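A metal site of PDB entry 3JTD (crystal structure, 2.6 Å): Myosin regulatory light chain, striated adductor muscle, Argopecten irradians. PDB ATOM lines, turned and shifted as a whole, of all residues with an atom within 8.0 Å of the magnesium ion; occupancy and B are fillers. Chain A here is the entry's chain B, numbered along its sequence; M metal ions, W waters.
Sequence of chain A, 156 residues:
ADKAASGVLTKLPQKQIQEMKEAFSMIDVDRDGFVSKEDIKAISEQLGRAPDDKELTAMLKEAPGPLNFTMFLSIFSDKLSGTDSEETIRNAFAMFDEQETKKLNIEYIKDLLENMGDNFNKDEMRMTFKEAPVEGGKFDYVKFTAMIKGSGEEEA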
ATOM      1  N   PHE A  24       0.960 -22.573  20.780  1.00  0.00           N
ATOM      2  CA  PHE A  24       0.978 -23.848  21.490  1.00  0.00           C
ATOM      3  C   PHE A  24       1.593 -23.720  22.864  1.00  0.00           C
ATOM      4  O   PHE A  24       1.047 -24.246  23.842  1.00  0.00           O
ATOM      5  CB  PHE A  24       1.774 -24.897  20.697  1.00  0.00           C
ATOM      6  CG  PHE A  24       1.853 -26.259  21.385  1.00  0.00           C
ATOM      7  CD1 PHE A  24       0.868 -27.225  21.174  1.00  0.00           C
ATOM      8  CD2 PHE A  24       2.910 -26.557  22.247  1.00  0.00           C
ATOM      9  CE1 PHE A  24       0.932 -28.473  21.815  1.00  0.00           C
ATOM     10  CE2 PHE A  24       2.971 -27.801  22.896  1.00  0.00           C
ATOM     11  CZ  PHE A  24       1.985 -28.767  22.685  1.00  0.00           C
ATOM     12  N   SER A  25       2.739 -23.055  22.954  1.00  0.00           N
ATOM     13  CA  SER A  25       3.373 -22.940  24.248  1.00  0.00           C
ATOM     14  C   SER A  25       2.574 -22.097  25.197  1.00  0.00           C
ATOM     15  O   SER A  25       2.671 -22.291  26.410  1.00  0.00           O
ATOM     16  CB  SER A  25       4.838 -22.430  24.142  1.00  0.00           C
ATOM     17  OG  SER A  25       5.130 -21.731  22.947  1.00  0.00           O
ATOM     18  N   ILE A  27      -0.625 -22.149  25.295  1.00  0.00           N
ATOM     19  CA  ILE A  27      -1.756 -22.996  25.661  1.00  0.00           C
ATOM     20  C   ILE A  27      -1.321 -24.123  26.601  1.00  0.00           C
ATOM     21  O   ILE A  27      -2.108 -24.605  27.405  1.00  0.00           O
ATOM     22  CB  ILE A  27      -2.423 -23.612  24.417  1.00  0.00           C
ATOM     23  CG1 ILE A  27      -2.782 -22.523  23.401  1.00  0.00           C
ATOM     24  CG2 ILE A  27      -3.666 -24.404  24.808  1.00  0.00           C
ATOM     25  CD1 ILE A  27      -3.206 -23.060  22.057  1.00  0.00           C
ATOM     26  N   ASP A  28      -0.078 -24.543  26.453  1.00  0.00           N
ATOM     27  CA  ASP A  28       0.487 -25.586  27.318  1.00  0.00           C
ATOM     28  C   ASP A  28       0.851 -24.960  28.627  1.00  0.00           C
ATOM     29  O   ASP A  28       2.013 -24.696  28.903  1.00  0.00           O
ATOM     30  CB  ASP A  28       1.685 -26.244  26.634  1.00  0.00           C
ATOM     31  CG  ASP A  28       2.330 -27.320  27.491  1.00  0.00           C
ATOM     32  OD1 ASP A  28       1.599 -27.995  28.242  1.00  0.00           O
ATOM     33  OD2 ASP A  28       3.566 -27.482  27.410  1.00  0.00           O
ATOM     34  N   VAL A  29      -0.158 -24.722  29.470  1.00  0.00           N
ATOM     35  CA  VAL A  29       0.052 -23.961  30.697  1.00  0.00           C
ATOM     36  C   VAL A  29       0.925 -24.561  31.782  1.00  0.00           C
ATOM     37  O   VAL A  29       1.406 -23.860  32.674  1.00  0.00           O
ATOM     38  CB  VAL A  29      -1.322 -23.590  31.291  1.00  0.00           C
ATOM     39  CG1 VAL A  29      -1.167 -23.226  32.763  1.00  0.00           C
ATOM     40  CG2 VAL A  29      -1.954 -22.452  30.510  1.00  0.00           C
ATOM     41  N   ASP A  30       1.137 -25.874  31.706  1.00  0.00           N
ATOM     42  CA  ASP A  30       1.861 -26.601  32.745  1.00  0.00           C
ATOM     43  C   ASP A  30       3.269 -26.994  32.318  1.00  0.00           C
ATOM     44  O   ASP A  30       4.043 -27.537  33.110  1.00  0.00           O
ATOM     45  CB  ASP A  30       1.076 -27.819  33.219  1.00  0.00           C
ATOM     46  CG  ASP A  30       1.180 -28.993  32.262  1.00  0.00           C
ATOM     47  OD1 ASP A  30       0.593 -30.048  32.561  1.00  0.00           O
ATOM     48  OD2 ASP A  30       1.842 -28.849  31.224  1.00  0.00           O
ATOM     49  N   ARG A  31       3.603 -26.729  31.068  1.00  0.00           N
ATOM     50  CA  ARG A  31       4.987 -26.501  30.667  1.00  0.00           C
ATOM     51  C   ARG A  31       5.700 -27.807  30.353  1.00  0.00           C
ATOM     52  O   ARG A  31       6.934 -27.843  30.279  1.00  0.00           O
ATOM     53  CB  ARG A  31       5.730 -25.745  31.760  1.00  0.00           C
ATOM     54  CG  ARG A  31       5.873 -24.263  31.516  1.00  0.00           C
ATOM     55  CD  ARG A  31       6.982 -23.692  32.372  1.00  0.00           C
ATOM     56  NE  ARG A  31       7.302 -24.533  33.521  1.00  0.00           N
ATOM     57  CZ  ARG A  31       7.732 -25.790  33.429  1.00  0.00           C
ATOM     58  NH1 ARG A  31       7.893 -26.356  32.250  1.00  0.00           N
ATOM     59  NH2 ARG A  31       7.991 -26.489  34.528  1.00  0.00           N
ATOM     60  N   ASP A  32       4.936 -28.880  30.159  1.00  0.00           N
ATOM     61  CA  ASP A  32       5.469 -30.234  30.163  1.00  0.00           C
ATOM     62  C   ASP A  32       5.555 -30.828  28.762  1.00  0.00           C
ATOM     63  O   ASP A  32       6.017 -31.951  28.579  1.00  0.00           O
ATOM     64  CB  ASP A  32       4.660 -31.147  31.089  1.00  0.00           C
ATOM     65  CG  ASP A  32       3.314 -31.558  30.505  1.00  0.00           C
ATOM     66  OD1 ASP A  32       2.575 -30.680  30.028  1.00  0.00           O
ATOM     67  OD2 ASP A  32       2.991 -32.757  30.520  1.00  0.00           O
ATOM     68  N   GLY A  33       5.090 -30.073  27.776  1.00  0.00           N
ATOM     69  CA  GLY A  33       5.202 -30.478  26.382  1.00  0.00           C
ATOM     70  C   GLY A  33       3.946 -31.118  25.807  1.00  0.00           C
ATOM     71  O   GLY A  33       3.913 -31.491  24.633  1.00  0.00           O
ATOM     72  N   PHE A  34       2.932 -31.263  26.652  1.00  0.00           N
ATOM     73  CA  PHE A  34       1.668 -31.852  26.232  1.00  0.00           C
ATOM     74  C   PHE A  34       0.511 -30.962  26.655  1.00  0.00           C
ATOM     75  O   PHE A  34       0.512 -30.410  27.757  1.00  0.00           O
ATOM     76  CB  PHE A  34       1.495 -33.254  26.840  1.00  0.00           C
ATOM     77  CG  PHE A  34       2.549 -34.230  26.409  1.00  0.00           C
ATOM     78  CD1 PHE A  34       2.332 -35.090  25.354  1.00  0.00           C
ATOM     79  CD2 PHE A  34       3.766 -34.303  27.078  1.00  0.00           C
ATOM     80  CE1 PHE A  34       3.292 -35.982  24.961  1.00  0.00           C
ATOM     81  CE2 PHE A  34       4.730 -35.204  26.690  1.00  0.00           C
ATOM     82  CZ  PHE A  34       4.504 -36.043  25.634  1.00  0.00           C
ATOM     83  N   VAL A  35      -0.478 -30.815  25.781  1.00  0.00           N
ATOM     84  CA  VAL A  35      -1.740 -30.154  26.162  1.00  0.00           C
ATOM     85  C   VAL A  35      -2.669 -31.098  26.889  1.00  0.00           C
ATOM     86  O   VAL A  35      -3.158 -32.060  26.314  1.00  0.00           O
ATOM     87  CB  VAL A  35      -2.484 -29.606  24.919  1.00  0.00           C
ATOM     88  CG1 VAL A  35      -3.749 -28.895  25.343  1.00  0.00           C
ATOM     89  CG2 VAL A  35      -1.589 -28.679  24.122  1.00  0.00           C
ATOM     90  N   SER A  36      -2.912 -30.828  28.167  1.00  0.00           N
ATOM     91  CA  SER A  36      -3.843 -31.624  28.959  1.00  0.00           C
ATOM     92  C   SER A  36      -5.267 -31.096  28.894  1.00  0.00           C
ATOM     93  O   SER A  36      -5.521 -30.042  28.309  1.00  0.00           O
ATOM     94  CB  SER A  36      -3.375 -31.694  30.413  1.00  0.00           C
ATOM     95  OG  SER A  36      -3.094 -30.402  30.923  1.00  0.00           O
ATOM     96  N   LYS A  37      -6.196 -31.829  29.497  1.00  0.00           N
ATOM     97  CA  LYS A  37      -7.557 -31.346  29.688  1.00  0.00           C
ATOM     98  C   LYS A  37      -7.603 -30.123  30.602  1.00  0.00           C
ATOM     99  O   LYS A  37      -8.507 -29.308  30.511  1.00  0.00           O
ATOM    100  CB  LYS A  37      -8.426 -32.460  30.273  1.00  0.00           C
ATOM    101  CG  LYS A  37      -9.821 -32.535  29.686  1.00  0.00           C
ATOM    102  CD  LYS A  37     -10.515 -33.828  30.095  1.00  0.00           C
ATOM    103  CE  LYS A  37     -12.031 -33.669  30.117  1.00  0.00           C
ATOM    104  NZ  LYS A  37     -12.438 -32.368  30.729  1.00  0.00           N
ATOM    105  N   GLU A  38      -6.610 -30.009  31.477  1.00  0.00           N
ATOM    106  CA  GLU A  38      -6.573 -28.957  32.461  1.00  0.00           C
ATOM    107  C   GLU A  38      -5.867 -27.727  31.915  1.00  0.00           C
ATOM    108  O   GLU A  38      -6.083 -26.621  32.397  1.00  0.00           O
ATOM    109  CB  GLU A  38      -5.848 -29.439  33.725  1.00  0.00           C
ATOM    110  CG  GLU A  38      -6.373 -30.734  34.304  1.00  0.00           C
ATOM    111  CD  GLU A  38      -5.433 -31.919  34.058  1.00  0.00           C
ATOM    112  OE1 GLU A  38      -4.248 -31.792  34.440  1.00  0.00           O
ATOM    113  OE2 GLU A  38      -5.865 -32.938  33.491  1.00  0.00           O
ATOM    114  N   ASP A  39      -5.000 -27.926  30.924  1.00  0.00           N
ATOM    115  CA  ASP A  39      -4.302 -26.796  30.320  1.00  0.00           C
ATOM    116  C   ASP A  39      -5.329 -25.957  29.560  1.00  0.00           C
ATOM    117  O   ASP A  39      -5.352 -24.726  29.656  1.00  0.00           O
ATOM    118  CB  ASP A  39      -3.222 -27.257  29.340  1.00  0.00           C
ATOM    119  CG  ASP A  39      -1.967 -27.763  30.023  1.00  0.00           C
ATOM    120  OD1 ASP A  39      -1.427 -27.046  30.900  1.00  0.00           O
ATOM    121  OD2 ASP A  39      -1.505 -28.869  29.661  1.00  0.00           O
ATOM    122  N   ILE A  40      -6.177 -26.634  28.800  1.00  0.00           N
ATOM    123  CA  ILE A  40      -7.181 -25.918  28.024  1.00  0.00           C
ATOM    124  C   ILE A  40      -8.092 -25.140  28.941  1.00  0.00           C
ATOM    125  O   ILE A  40      -8.312 -23.954  28.723  1.00  0.00           O
ATOM    126  CB  ILE A  40      -8.010 -26.871  27.140  1.00  0.00           C
ATOM    127  CG1 ILE A  40      -7.085 -27.653  26.206  1.00  0.00           C
ATOM    128  CG2 ILE A  40      -9.024 -26.078  26.314  1.00  0.00           C
ATOM    129  CD1 ILE A  40      -7.789 -28.723  25.389  1.00  0.00           C
ATOM    130  N   LEU A  67      -1.140 -35.495  22.849  1.00  0.00           N
ATOM    131  CA  LEU A  67      -1.080 -34.203  22.174  1.00  0.00           C
ATOM    132  C   LEU A  67       0.173 -33.341  22.334  1.00  0.00           C
ATOM    133  O   LEU A  67       0.265 -32.503  23.230  1.00  0.00           O
ATOM    134  CB  LEU A  67      -2.326 -33.378  22.549  1.00  0.00           C
ATOM    135  CG  LEU A  67      -2.847 -32.300  21.587  1.00  0.00           C
ATOM    136  CD1 LEU A  67      -4.283 -31.965  21.977  1.00  0.00           C
ATOM    137  CD2 LEU A  67      -1.981 -31.047  21.617  1.00  0.00           C
HETATM  138 MG    MG M   1       0.770 -29.347  29.295  1.00  0.00          MG
HETATM  139  O   HOH W   1      -0.127 -31.034  30.308  1.00  0.00           O
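Of the 17 residues printed, 5 come within 4 Å of the magnesium ion. The nearest printed residue that does not touch the magnesium ion is Val 35 (4.01 Å).
The backbone carbonyl oxygen (O) of Phe 34 binds the magnesium ion (1.9 Å). The side-chain carboxylate (OD1) of Asp 28 binds the magnesium ion (1.9 Å). Water W1 binds the magnesium ion (2.2 Å). OD2 of Asp 30 is bound to the magnesium ion, at 2.3 Å. The magnesium ion is bound by OD2 of Asp 39. OD1 of Asp 32 binds the magnesium ion, at 2.4 Å.
Water W1 lies within hydrogen-bond range of OD1 of Asp 30 (2.6 Å) and OG of Ser 36 (3.1 Å).
The backbone NH (N) of Val 29 is in hydrogen-bond range of the side-chain carboxylate (OD1) of Asp 39 (3.0 Å). The backbone NH (N) of Asp 39 sits close to the side-chain hydroxyl (OG) of Ser 36 (3.1 Å). The side-chain carboxylate of Asp 28 is in hydrogen-bond range of the backbone NH of Gly 33 (3.0 Å).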
